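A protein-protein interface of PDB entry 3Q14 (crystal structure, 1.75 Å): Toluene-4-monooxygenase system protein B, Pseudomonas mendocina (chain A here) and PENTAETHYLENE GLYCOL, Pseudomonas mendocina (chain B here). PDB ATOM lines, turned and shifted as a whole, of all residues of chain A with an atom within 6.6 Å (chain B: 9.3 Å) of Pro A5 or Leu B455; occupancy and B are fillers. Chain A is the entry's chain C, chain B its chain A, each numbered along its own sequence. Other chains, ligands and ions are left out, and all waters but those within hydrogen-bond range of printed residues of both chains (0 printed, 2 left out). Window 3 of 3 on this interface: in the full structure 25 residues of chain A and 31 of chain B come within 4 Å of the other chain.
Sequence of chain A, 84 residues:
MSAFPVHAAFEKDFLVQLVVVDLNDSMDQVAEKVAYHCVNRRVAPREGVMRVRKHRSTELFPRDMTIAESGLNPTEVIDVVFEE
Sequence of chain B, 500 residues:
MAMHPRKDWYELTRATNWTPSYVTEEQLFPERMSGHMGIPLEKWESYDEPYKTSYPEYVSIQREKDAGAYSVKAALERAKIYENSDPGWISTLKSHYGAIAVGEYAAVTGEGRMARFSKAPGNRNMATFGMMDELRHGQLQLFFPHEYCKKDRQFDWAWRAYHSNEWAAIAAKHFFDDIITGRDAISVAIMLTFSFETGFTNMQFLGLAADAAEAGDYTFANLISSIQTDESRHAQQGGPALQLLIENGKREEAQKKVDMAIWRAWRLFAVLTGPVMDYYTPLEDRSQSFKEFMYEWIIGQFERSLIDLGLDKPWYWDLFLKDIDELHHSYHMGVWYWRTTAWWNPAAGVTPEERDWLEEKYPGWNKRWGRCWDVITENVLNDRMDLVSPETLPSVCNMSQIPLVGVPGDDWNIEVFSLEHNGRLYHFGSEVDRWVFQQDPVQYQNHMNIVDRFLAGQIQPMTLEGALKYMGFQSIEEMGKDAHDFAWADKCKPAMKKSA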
ATOM      1  N   ALA A   3      -1.067   4.414   5.554  1.00  0.00           N
ATOM      2  CA  ALA A   3      -0.253   4.937   4.460  1.00  0.00           C
ATOM      3  C   ALA A   3      -0.028   6.420   4.705  1.00  0.00           C
ATOM      4  O   ALA A   3      -0.941   7.134   5.126  1.00  0.00           O
ATOM      5  CB  ALA A   3      -0.944   4.729   3.126  1.00  0.00           C
ATOM      6  N   PHE A   4       1.187   6.878   4.434  1.00  0.00           N
ATOM      7  CA  PHE A   4       1.570   8.251   4.720  1.00  0.00           C
ATOM      8  C   PHE A   4       2.460   8.754   3.587  1.00  0.00           C
ATOM      9  O   PHE A   4       3.647   8.436   3.547  1.00  0.00           O
ATOM     10  CB  PHE A   4       2.326   8.306   6.049  1.00  0.00           C
ATOM     11  CG  PHE A   4       2.542   9.697   6.578  1.00  0.00           C
ATOM     12  CD1 PHE A   4       1.698  10.219   7.545  1.00  0.00           C
ATOM     13  CD2 PHE A   4       3.594  10.478   6.120  1.00  0.00           C
ATOM     14  CE1 PHE A   4       1.895  11.500   8.039  1.00  0.00           C
ATOM     15  CE2 PHE A   4       3.795  11.761   6.611  1.00  0.00           C
ATOM     16  CZ  PHE A   4       2.943  12.271   7.570  1.00  0.00           C
ATOM     17  N   PRO A   5       1.884   9.527   2.654  1.00  0.00           N
ATOM     18  CA  PRO A   5       2.673  10.022   1.522  1.00  0.00           C
ATOM     19  C   PRO A   5       3.589  11.172   1.919  1.00  0.00           C
ATOM     20  O   PRO A   5       3.156  12.094   2.612  1.00  0.00           O
ATOM     21  CB  PRO A   5       1.603  10.530   0.559  1.00  0.00           C
ATOM     22  CG  PRO A   5       0.492  10.966   1.444  1.00  0.00           C
ATOM     23  CD  PRO A   5       0.479   9.964   2.576  1.00  0.00           C
ATOM     24  N   VAL A   6       4.850  11.096   1.502  1.00  0.00           N
ATOM     25  CA  VAL A   6       5.780  12.208   1.653  1.00  0.00           C
ATOM     26  C   VAL A   6       6.448  12.481   0.312  1.00  0.00           C
ATOM     27  O   VAL A   6       6.382  11.664  -0.598  1.00  0.00           O
ATOM     28  CB  VAL A   6       6.869  11.919   2.705  1.00  0.00           C
ATOM     29  CG1 VAL A   6       6.238  11.528   4.017  1.00  0.00           C
ATOM     30  CG2 VAL A   6       7.817  10.823   2.216  1.00  0.00           C
ATOM     31  N   HIS A   7       7.075  13.642   0.197  1.00  0.00           N
ATOM     32  CA  HIS A   7       7.872  13.969  -0.976  1.00  0.00           C
ATOM     33  C   HIS A   7       9.311  13.998  -0.486  1.00  0.00           C
ATOM     34  O   HIS A   7       9.624  14.711   0.461  1.00  0.00           O
ATOM     35  CB  HIS A   7       7.468  15.335  -1.536  1.00  0.00           C
ATOM     36  CG  HIS A   7       6.112  15.349  -2.175  1.00  0.00           C
ATOM     37  ND1 HIS A   7       5.036  16.018  -1.629  1.00  0.00           N
ATOM     38  CD2 HIS A   7       5.655  14.769  -3.311  1.00  0.00           C
ATOM     39  CE1 HIS A   7       3.978  15.855  -2.406  1.00  0.00           C
ATOM     40  NE2 HIS A   7       4.329  15.107  -3.436  1.00  0.00           N
ATOM     41  N   LEU A  18       7.596  11.250  -4.984  1.00  0.00           N
ATOM     42  CA  LEU A  18       6.561  10.780  -4.084  1.00  0.00           C
ATOM     43  C   LEU A  18       6.971   9.421  -3.536  1.00  0.00           C
ATOM     44  O   LEU A  18       7.249   8.492  -4.296  1.00  0.00           O
ATOM     45  CB  LEU A  18       5.226  10.661  -4.816  1.00  0.00           C
ATOM     46  CG  LEU A  18       4.133   9.937  -4.028  1.00  0.00           C
ATOM     47  CD1 LEU A  18       3.709  10.769  -2.815  1.00  0.00           C
ATOM     48  CD2 LEU A  18       2.940   9.632  -4.923  1.00  0.00           C
ATOM     49  N   VAL A  19       7.034   9.311  -2.215  1.00  0.00           N
ATOM     50  CA  VAL A  19       7.276   8.025  -1.580  1.00  0.00           C
ATOM     51  C   VAL A  19       6.234   7.824  -0.502  1.00  0.00           C
ATOM     52  O   VAL A  19       6.081   8.661   0.384  1.00  0.00           O
ATOM     53  CB  VAL A  19       8.668   7.957  -0.947  1.00  0.00           C
ATOM     54  CG1 VAL A  19       8.868   6.611  -0.276  1.00  0.00           C
ATOM     55  CG2 VAL A  19       9.730   8.181  -2.010  1.00  0.00           C
ATOM     56  N   VAL A  20       5.503   6.721  -0.576  1.00  0.00           N
ATOM     57  CA  VAL A  20       4.500   6.463   0.441  1.00  0.00           C
ATOM     58  C   VAL A  20       5.097   5.592   1.531  1.00  0.00           C
ATOM     59  O   VAL A  20       5.512   4.456   1.279  1.00  0.00           O
ATOM     60  CB  VAL A  20       3.242   5.806  -0.142  1.00  0.00           C
ATOM     61  CG1 VAL A  20       2.195   5.603   0.952  1.00  0.00           C
ATOM     62  CG2 VAL A  20       2.686   6.658  -1.265  1.00  0.00           C
ATOM     63  N   VAL A  21       5.154   6.140   2.739  1.00  0.00           N
ATOM     64  CA  VAL A  21       5.674   5.414   3.884  1.00  0.00           C
ATOM     65  C   VAL A  21       4.526   5.044   4.819  1.00  0.00           C
ATOM     66  O   VAL A  21       3.351   5.178   4.462  1.00  0.00           O
ATOM     67  CB  VAL A  21       6.747   6.236   4.629  1.00  0.00           C
ATOM     68  CG1 VAL A  21       7.869   6.626   3.665  1.00  0.00           C
ATOM     69  CG2 VAL A  21       6.130   7.480   5.255  1.00  0.00           C
ATOM     70  N   ASN A  73       3.499  16.311   8.560  1.00  0.00           N
ATOM     71  CA  ASN A  73       2.184  16.187   7.947  1.00  0.00           C
ATOM     72  C   ASN A  73       2.295  15.501   6.591  1.00  0.00           C
ATOM     73  O   ASN A  73       3.327  15.600   5.927  1.00  0.00           O
ATOM     74  CB  ASN A  73       1.528  17.556   7.786  1.00  0.00           C
ATOM     75  CG  ASN A  73       1.278  18.239   9.123  1.00  0.00           C
ATOM     76  OD1 ASN A  73       1.097  17.575  10.142  1.00  0.00           O
ATOM     77  ND2 ASN A  73       1.271  19.565   9.122  1.00  0.00           N
ATOM     78  N   PRO A  74       1.237  14.792   6.181  1.00  0.00           N
ATOM     79  CA  PRO A  74       1.268  14.125   4.878  1.00  0.00           C
ATOM     80  C   PRO A  74       1.615  15.133   3.786  1.00  0.00           C
ATOM     81  O   PRO A  74       1.239  16.299   3.894  1.00  0.00           O
ATOM     82  CB  PRO A  74      -0.169  13.627   4.706  1.00  0.00           C
ATOM     83  CG  PRO A  74      -0.687  13.482   6.096  1.00  0.00           C
ATOM     84  CD  PRO A  74      -0.031  14.566   6.896  1.00  0.00           C
ATOM     85  N   THR A  75       2.336  14.673   2.770  1.00  0.00           N
ATOM     86  CA  THR A  75       2.759  15.475   1.617  1.00  0.00           C
ATOM     87  C   THR A  75       3.779  16.576   1.924  1.00  0.00           C
ATOM     88  O   THR A  75       4.094  17.385   1.054  1.00  0.00           O
ATOM     89  CB  THR A  75       1.568  16.052   0.803  1.00  0.00           C
ATOM     90  OG1 THR A  75       0.999  17.179   1.482  1.00  0.00           O
ATOM     91  CG2 THR A  75       0.502  14.989   0.579  1.00  0.00           C
ATOM     92  N   GLU A  76       4.305  16.601   3.144  1.00  0.00           N
ATOM     93  CA  GLU A  76       5.439  17.473   3.440  1.00  0.00           C
ATOM     94  C   GLU A  76       6.717  16.927   2.792  1.00  0.00           C
ATOM     95  O   GLU A  76       6.796  15.747   2.436  1.00  0.00           O
ATOM     96  CB  GLU A  76       5.604  17.677   4.954  1.00  0.00           C
ATOM     97  CG  GLU A  76       4.553  18.629   5.532  1.00  0.00           C
ATOM     98  CD  GLU A  76       4.667  18.853   7.041  1.00  0.00           C
ATOM     99  OE1 GLU A  76       5.572  18.287   7.687  1.00  0.00           O
ATOM    100  OE2 GLU A  76       3.833  19.610   7.583  1.00  0.00           O
ATOM    101  N   THR B 392       7.965   4.777  -8.967  1.00  0.00           N
ATOM    102  CA  THR B 392       7.167   5.768  -8.259  1.00  0.00           C
ATOM    103  C   THR B 392       6.976   7.024  -9.107  1.00  0.00           C
ATOM    104  O   THR B 392       7.549   7.133 -10.195  1.00  0.00           O
ATOM    105  CB  THR B 392       7.789   6.139  -6.906  1.00  0.00           C
ATOM    106  OG1 THR B 392       6.826   6.854  -6.122  1.00  0.00           O
ATOM    107  CG2 THR B 392       9.039   6.992  -7.104  1.00  0.00           C
ATOM    108  N   LEU B 393       6.161   7.952  -8.614  1.00  0.00           N
ATOM    109  CA  LEU B 393       5.920   9.228  -9.298  1.00  0.00           C
ATOM    110  C   LEU B 393       6.924  10.286  -8.855  1.00  0.00           C
ATOM    111  O   LEU B 393       7.345  10.304  -7.701  1.00  0.00           O
ATOM    112  CB  LEU B 393       4.518   9.764  -8.974  1.00  0.00           C
ATOM    113  CG  LEU B 393       3.251   9.159  -9.583  1.00  0.00           C
ATOM    114  CD1 LEU B 393       3.219   9.396 -11.082  1.00  0.00           C
ATOM    115  CD2 LEU B 393       3.160   7.677  -9.268  1.00  0.00           C
ATOM    116  N   PRO B 394       7.296  11.189  -9.770  1.00  0.00           N
ATOM    117  CA  PRO B 394       8.056  12.368  -9.348  1.00  0.00           C
ATOM    118  C   PRO B 394       7.133  13.356  -8.645  1.00  0.00           C
ATOM    119  O   PRO B 394       5.931  13.351  -8.904  1.00  0.00           O
ATOM    120  CB  PRO B 394       8.538  12.965 -10.674  1.00  0.00           C
ATOM    121  CG  PRO B 394       7.542  12.504 -11.682  1.00  0.00           C
ATOM    122  CD  PRO B 394       7.083  11.146 -11.228  1.00  0.00           C
ATOM    123  N   SER B 395       7.678  14.176  -7.751  1.00  0.00           N
ATOM    124  CA  SER B 395       6.894  15.247  -7.157  1.00  0.00           C
ATOM    125  C   SER B 395       6.788  16.374  -8.182  1.00  0.00           C
ATOM    126  O   SER B 395       7.752  16.648  -8.897  1.00  0.00           O
ATOM    127  CB  SER B 395       7.565  15.743  -5.882  1.00  0.00           C
ATOM    128  OG  SER B 395       7.836  14.640  -5.030  1.00  0.00           O
ATOM    129  N   VAL B 396       5.630  17.025  -8.239  1.00  0.00           N
ATOM    130  CA  VAL B 396       5.320  17.950  -9.332  1.00  0.00           C
ATOM    131  C   VAL B 396       5.011  19.365  -8.854  1.00  0.00           C
ATOM    132  O   VAL B 396       4.329  19.556  -7.845  1.00  0.00           O
ATOM    133  CB  VAL B 396       4.131  17.430 -10.157  1.00  0.00           C
ATOM    134  CG1 VAL B 396       3.719  18.438 -11.228  1.00  0.00           C
ATOM    135  CG2 VAL B 396       4.490  16.092 -10.802  1.00  0.00           C
ATOM    136  N   LEU B 425      -1.631  22.428   1.210  1.00  0.00           N
ATOM    137  CA  LEU B 425      -0.186  22.566   1.065  1.00  0.00           C
ATOM    138  C   LEU B 425       0.241  22.427  -0.401  1.00  0.00           C
ATOM    139  O   LEU B 425       0.043  21.380  -1.023  1.00  0.00           O
ATOM    140  CB  LEU B 425       0.533  21.519   1.917  1.00  0.00           C
ATOM    141  CG  LEU B 425       2.060  21.551   1.853  1.00  0.00           C
ATOM    142  CD1 LEU B 425       2.565  22.920   2.300  1.00  0.00           C
ATOM    143  CD2 LEU B 425       2.669  20.446   2.697  1.00  0.00           C
ATOM    144  N   HIS B 427       3.348  22.964  -3.470  1.00  0.00           N
ATOM    145  CA  HIS B 427       4.797  22.877  -3.619  1.00  0.00           C
ATOM    146  C   HIS B 427       5.207  23.448  -4.964  1.00  0.00           C
ATOM    147  O   HIS B 427       4.623  23.102  -5.989  1.00  0.00           O
ATOM    148  CB  HIS B 427       5.259  21.414  -3.531  1.00  0.00           C
ATOM    149  CG  HIS B 427       4.883  20.740  -2.248  1.00  0.00           C
ATOM    150  ND1 HIS B 427       5.415  21.105  -1.029  1.00  0.00           N
ATOM    151  CD2 HIS B 427       4.014  19.733  -1.992  1.00  0.00           C
ATOM    152  CE1 HIS B 427       4.897  20.345  -0.079  1.00  0.00           C
ATOM    153  NE2 HIS B 427       4.045  19.503  -0.637  1.00  0.00           N
ATOM    154  N   MET B 448      -5.662  20.998  -9.329  1.00  0.00           N
ATOM    155  CA  MET B 448      -4.937  19.863  -8.780  1.00  0.00           C
ATOM    156  C   MET B 448      -3.986  19.336  -9.832  1.00  0.00           C
ATOM    157  O   MET B 448      -4.396  19.044 -10.961  1.00  0.00           O
ATOM    158  CB  MET B 448      -5.908  18.763  -8.348  1.00  0.00           C
ATOM    159  CG  MET B 448      -6.902  19.253  -7.297  1.00  0.00           C
ATOM    160  SD  MET B 448      -8.004  17.944  -6.741  1.00  0.00           S
ATOM    161  CE  MET B 448      -6.813  16.718  -6.208  1.00  0.00           C
ATOM    162  N   ASN B 449      -2.710  19.223  -9.471  1.00  0.00           N
ATOM    163  CA  ASN B 449      -1.747  18.650 -10.399  1.00  0.00           C
ATOM    164  C   ASN B 449      -1.888  17.126 -10.423  1.00  0.00           C
ATOM    165  O   ASN B 449      -2.671  16.549  -9.657  1.00  0.00           O
ATOM    166  CB  ASN B 449      -0.307  19.164 -10.149  1.00  0.00           C
ATOM    167  CG  ASN B 449       0.373  18.532  -8.941  1.00  0.00           C
ATOM    168  OD1 ASN B 449       0.009  17.451  -8.487  1.00  0.00           O
ATOM    169  ND2 ASN B 449       1.402  19.206  -8.436  1.00  0.00           N
ATOM    170  N   ILE B 450      -1.174  16.472 -11.322  1.00  0.00           N
ATOM    171  CA  ILE B 450      -1.409  15.046 -11.536  1.00  0.00           C
ATOM    172  C   ILE B 450      -1.119  14.210 -10.287  1.00  0.00           C
ATOM    173  O   ILE B 450      -1.807  13.224 -10.023  1.00  0.00           O
ATOM    174  CB  ILE B 450      -0.626  14.532 -12.764  1.00  0.00           C
ATOM    175  CG1 ILE B 450      -1.020  13.094 -13.093  1.00  0.00           C
ATOM    176  CG2 ILE B 450       0.872  14.663 -12.539  1.00  0.00           C
ATOM    177  CD1 ILE B 450      -0.798  12.747 -14.547  1.00  0.00           C
ATOM    178  N   VAL B 451      -0.113  14.618  -9.516  1.00  0.00           N
ATOM    179  CA  VAL B 451       0.228  13.942  -8.264  1.00  0.00           C
ATOM    180  C   VAL B 451      -0.858  14.169  -7.201  1.00  0.00           C
ATOM    181  O   VAL B 451      -1.219  13.249  -6.460  1.00  0.00           O
ATOM    182  CB  VAL B 451       1.601  14.421  -7.731  1.00  0.00           C
ATOM    183  CG1 VAL B 451       1.738  14.140  -6.244  1.00  0.00           C
ATOM    184  CG2 VAL B 451       2.736  13.788  -8.524  1.00  0.00           C
ATOM    185  N   ASP B 452      -1.365  15.399  -7.130  1.00  0.00           N
ATOM    186  CA  ASP B 452      -2.513  15.717  -6.281  1.00  0.00           C
ATOM    187  C   ASP B 452      -3.684  14.797  -6.609  1.00  0.00           C
ATOM    188  O   ASP B 452      -4.340  14.275  -5.714  1.00  0.00           O
ATOM    189  CB  ASP B 452      -2.974  17.164  -6.493  1.00  0.00           C
ATOM    190  CG  ASP B 452      -1.942  18.188  -6.052  1.00  0.00           C
ATOM    191  OD1 ASP B 452      -1.215  17.939  -5.062  1.00  0.00           O
ATOM    192  OD2 ASP B 452      -1.872  19.257  -6.699  1.00  0.00           O
ATOM    193  N   ARG B 453      -3.961  14.613  -7.898  1.00  0.00           N
ATOM    194  CA  ARG B 453      -5.060  13.739  -8.305  1.00  0.00           C
ATOM    195  C   ARG B 453      -4.794  12.283  -7.904  1.00  0.00           C
ATOM    196  O   ARG B 453      -5.691  11.572  -7.444  1.00  0.00           O
ATOM    197  CB  ARG B 453      -5.295  13.834  -9.818  1.00  0.00           C
ATOM    198  CG  ARG B 453      -5.574  15.252 -10.273  1.00  0.00           C
ATOM    199  CD  ARG B 453      -5.755  15.340 -11.775  1.00  0.00           C
ATOM    200  NE  ARG B 453      -5.601  16.729 -12.188  1.00  0.00           N
ATOM    201  CZ  ARG B 453      -5.775  17.182 -13.422  1.00  0.00           C
ATOM    202  NH1 ARG B 453      -6.128  16.354 -14.405  1.00  0.00           N
ATOM    203  NH2 ARG B 453      -5.596  18.476 -13.666  1.00  0.00           N
ATOM    204  N   PHE B 454      -3.550  11.851  -8.082  1.00  0.00           N
ATOM    205  CA  PHE B 454      -3.137  10.487  -7.755  1.00  0.00           C
ATOM    206  C   PHE B 454      -3.366  10.214  -6.271  1.00  0.00           C
ATOM    207  O   PHE B 454      -3.879   9.157  -5.888  1.00  0.00           O
ATOM    208  CB  PHE B 454      -1.660  10.303  -8.134  1.00  0.00           C
ATOM    209  CG  PHE B 454      -1.157   8.893  -8.007  1.00  0.00           C
ATOM    210  CD1 PHE B 454      -1.342   7.978  -9.033  1.00  0.00           C
ATOM    211  CD2 PHE B 454      -0.471   8.491  -6.875  1.00  0.00           C
ATOM    212  CE1 PHE B 454      -0.866   6.680  -8.925  1.00  0.00           C
ATOM    213  CE2 PHE B 454       0.007   7.193  -6.756  1.00  0.00           C
ATOM    214  CZ  PHE B 454      -0.191   6.286  -7.783  1.00  0.00           C
ATOM    215  N   LEU B 455      -3.010  11.184  -5.434  1.00  0.00           N
ATOM    216  CA  LEU B 455      -3.156  11.035  -3.988  1.00  0.00           C
ATOM    217  C   LEU B 455      -4.603  11.162  -3.511  1.00  0.00           C
ATOM    218  O   LEU B 455      -4.956  10.649  -2.438  1.00  0.00           O
ATOM    219  CB  LEU B 455      -2.278  12.051  -3.258  1.00  0.00           C
ATOM    220  CG  LEU B 455      -0.773  11.829  -3.418  1.00  0.00           C
ATOM    221  CD1 LEU B 455       0.003  12.939  -2.707  1.00  0.00           C
ATOM    222  CD2 LEU B 455      -0.387  10.461  -2.883  1.00  0.00           C
ATOM    223  N   ALA B 456      -5.429  11.847  -4.300  1.00  0.00           N
ATOM    224  CA  ALA B 456      -6.838  12.069  -3.964  1.00  0.00           C
ATOM    225  C   ALA B 456      -7.763  10.960  -4.468  1.00  0.00           C
ATOM    226  O   ALA B 456      -8.976  11.025  -4.282  1.00  0.00           O
ATOM    227  CB  ALA B 456      -7.305  13.416  -4.505  1.00  0.00           C
ATOM    228  N   GLY B 457      -7.198   9.958  -5.128  1.00  0.00           N
ATOM    229  CA  GLY B 457      -7.988   8.824  -5.584  1.00  0.00           C
ATOM    230  C   GLY B 457      -8.665   8.996  -6.935  1.00  0.00           C
ATOM    231  O   GLY B 457      -9.550   8.217  -7.289  1.00  0.00           O
ATOM    232  N   GLN B 458      -8.251  10.003  -7.698  1.00  0.00           N
ATOM    233  CA  GLN B 458      -8.852  10.257  -9.007  1.00  0.00           C
ATOM    234  C   GLN B 458      -8.255   9.382 -10.108  1.00  0.00           C
ATOM    235  O   GLN B 458      -8.810   9.282 -11.207  1.00  0.00           O
ATOM    236  CB  GLN B 458      -8.712  11.733  -9.391  1.00  0.00           C
ATOM    237  CG  GLN B 458      -9.529  12.671  -8.529  1.00  0.00           C
ATOM    238  CD  GLN B 458      -9.231  14.131  -8.814  1.00  0.00           C
ATOM    239  OE1 GLN B 458      -9.237  14.962  -7.907  1.00  0.00           O
ATOM    240  NE2 GLN B 458      -8.976  14.452 -10.081  1.00  0.00           N
ATOM    241  N   ILE B 459      -7.121   8.755  -9.811  1.00  0.00           N
ATOM    242  CA  ILE B 459      -6.426   7.927 -10.795  1.00  0.00           C
ATOM    243  C   ILE B 459      -6.454   6.475 -10.331  1.00  0.00           C
ATOM    244  O   ILE B 459      -5.800   6.111  -9.350  1.00  0.00           O
ATOM    245  CB  ILE B 459      -4.968   8.403 -10.999  1.00  0.00           C
ATOM    246  CG1 ILE B 459      -4.960   9.835 -11.544  1.00  0.00           C
ATOM    247  CG2 ILE B 459      -4.195   7.439 -11.907  1.00  0.00           C
ATOM    248  CD1 ILE B 459      -3.566  10.462 -11.658  1.00  0.00           C
ATOM    249  N   GLN B 460      -7.237   5.658 -11.030  1.00  0.00           N
ATOM    250  CA  GLN B 460      -7.425   4.263 -10.646  1.00  0.00           C
ATOM    251  C   GLN B 460      -7.129   3.315 -11.801  1.00  0.00           C
ATOM    252  O   GLN B 460      -7.556   3.553 -12.932  1.00  0.00           O
ATOM    253  CB  GLN B 460      -8.851   4.049 -10.145  1.00  0.00           C
ATOM    254  CG  GLN B 460      -9.195   4.884  -8.924  1.00  0.00           C
ATOM    255  CD  GLN B 460      -8.414   4.453  -7.694  1.00  0.00           C
ATOM    256  OE1 GLN B 460      -7.946   3.313  -7.613  1.00  0.00           O
ATOM    257  NE2 GLN B 460      -8.264   5.362  -6.736  1.00  0.00           N
ATOM    258  N   MET B 462      -4.180   2.889  -8.644  1.00  0.00           N
ATOM    259  CA  MET B 462      -3.038   3.710  -8.247  1.00  0.00           C
ATOM    260  C   MET B 462      -1.715   2.995  -8.497  1.00  0.00           C
ATOM    261  O   MET B 462      -1.044   2.563  -7.564  1.00  0.00           O
ATOM    262  CB  MET B 462      -3.148   4.105  -6.778  1.00  0.00           C
ATOM    263  CG  MET B 462      -4.255   5.104  -6.494  1.00  0.00           C
ATOM    264  SD  MET B 462      -4.315   5.584  -4.753  1.00  0.00           S
ATOM    265  CE  MET B 462      -2.731   6.394  -4.542  1.00  0.00           C
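The side-chain hydroxyl (OG1) of Thr B392 sits at hydrogen-bond distance from the backbone carbonyl oxygen (O) of Leu A18 (2.5 Å).
The backbone carbonyl oxygen (O) of Leu B393 lies within hydrogen-bond range of the backbone NH (N) of Leu A18 (2.9 Å).
NE2 of His B427 sits at hydrogen-bond distance from O of Thr A75 (2.7 Å).
N of Leu A18 sits at hydrogen-bond distance from OG of Ser B395, 3.4 Å away.
A ring nitrogen (ND1) of His A7 sits at hydrogen-bond distance from the backbone carbonyl oxygen (O) of Thr A75 (3.2 Å).
The backbone NH (N) of Thr A75 lies within hydrogen-bond range of the backbone carbonyl oxygen (O) of Pro A5, at 2.7 Å.
The side-chain amide oxygen (OD1) of Asn B449 sits at hydrogen-bond distance from the backbone NH (N) of Val B451, at 3.0 Å.
The backbone NH (N) of His A7 sits at hydrogen-bond distance from the backbone carbonyl oxygen (O) of Glu A76 (3.1 Å).
The side-chain amide nitrogen of Asn A73 sits at hydrogen-bond distance from the side-chain carboxylate of Glu A76 (3.0 Å).
Among the printed residues, merely in contact across the chains: His A7 with Ser B395 (2.8 Å), Thr A75 with Leu B425 (3.8 Å), His A7 with His B427 (3.8 Å), Glu A76 with Leu B425 (3.9 Å), Thr A75 with Leu B455 (3.9 Å), His A7 with Val B451 (3.9 Å), Pro A5 with Leu B455 (3.98 Å) and Leu A18 with Leu B455 (3.99 Å).
Pro A5 touches one residue of chain B.
Of the printed residues of chain B, Glu A76 touches Leu B425.
Printed residues of chain A within 4 Å of Thr B392: Leu A18.
Of the printed residues of chain A, Leu B455 touches Pro A5, Leu A18 and Thr A75.
The nearest residue of chain B that does not touch Pro A5 is Val B451 (7.7 Å).
Of the 13 printed residues of chain A, 5 touch a printed residue of chain B.
Printed residues of chain A that touch a printed residue of chain B: Pro A5, His A7, Leu A18, Thr A75 and Glu A76.
Hydrophobic or aromatic side chains of chain A that line the printed part of chain B: Pro A5, His A7 and Leu A18.
Of the 21 printed residues of chain B, 7 touch a printed residue of chain A.
Hydrophobic or aromatic side chains of chain B within 4 Å of the printed part of chain A: Leu B425, His B427, Val B451 and Leu B455.
Among the printed residues, no Asp or Glu carboxylate lies within 4 Å of a Lys or Arg side-chain nitrogen of the other chain.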
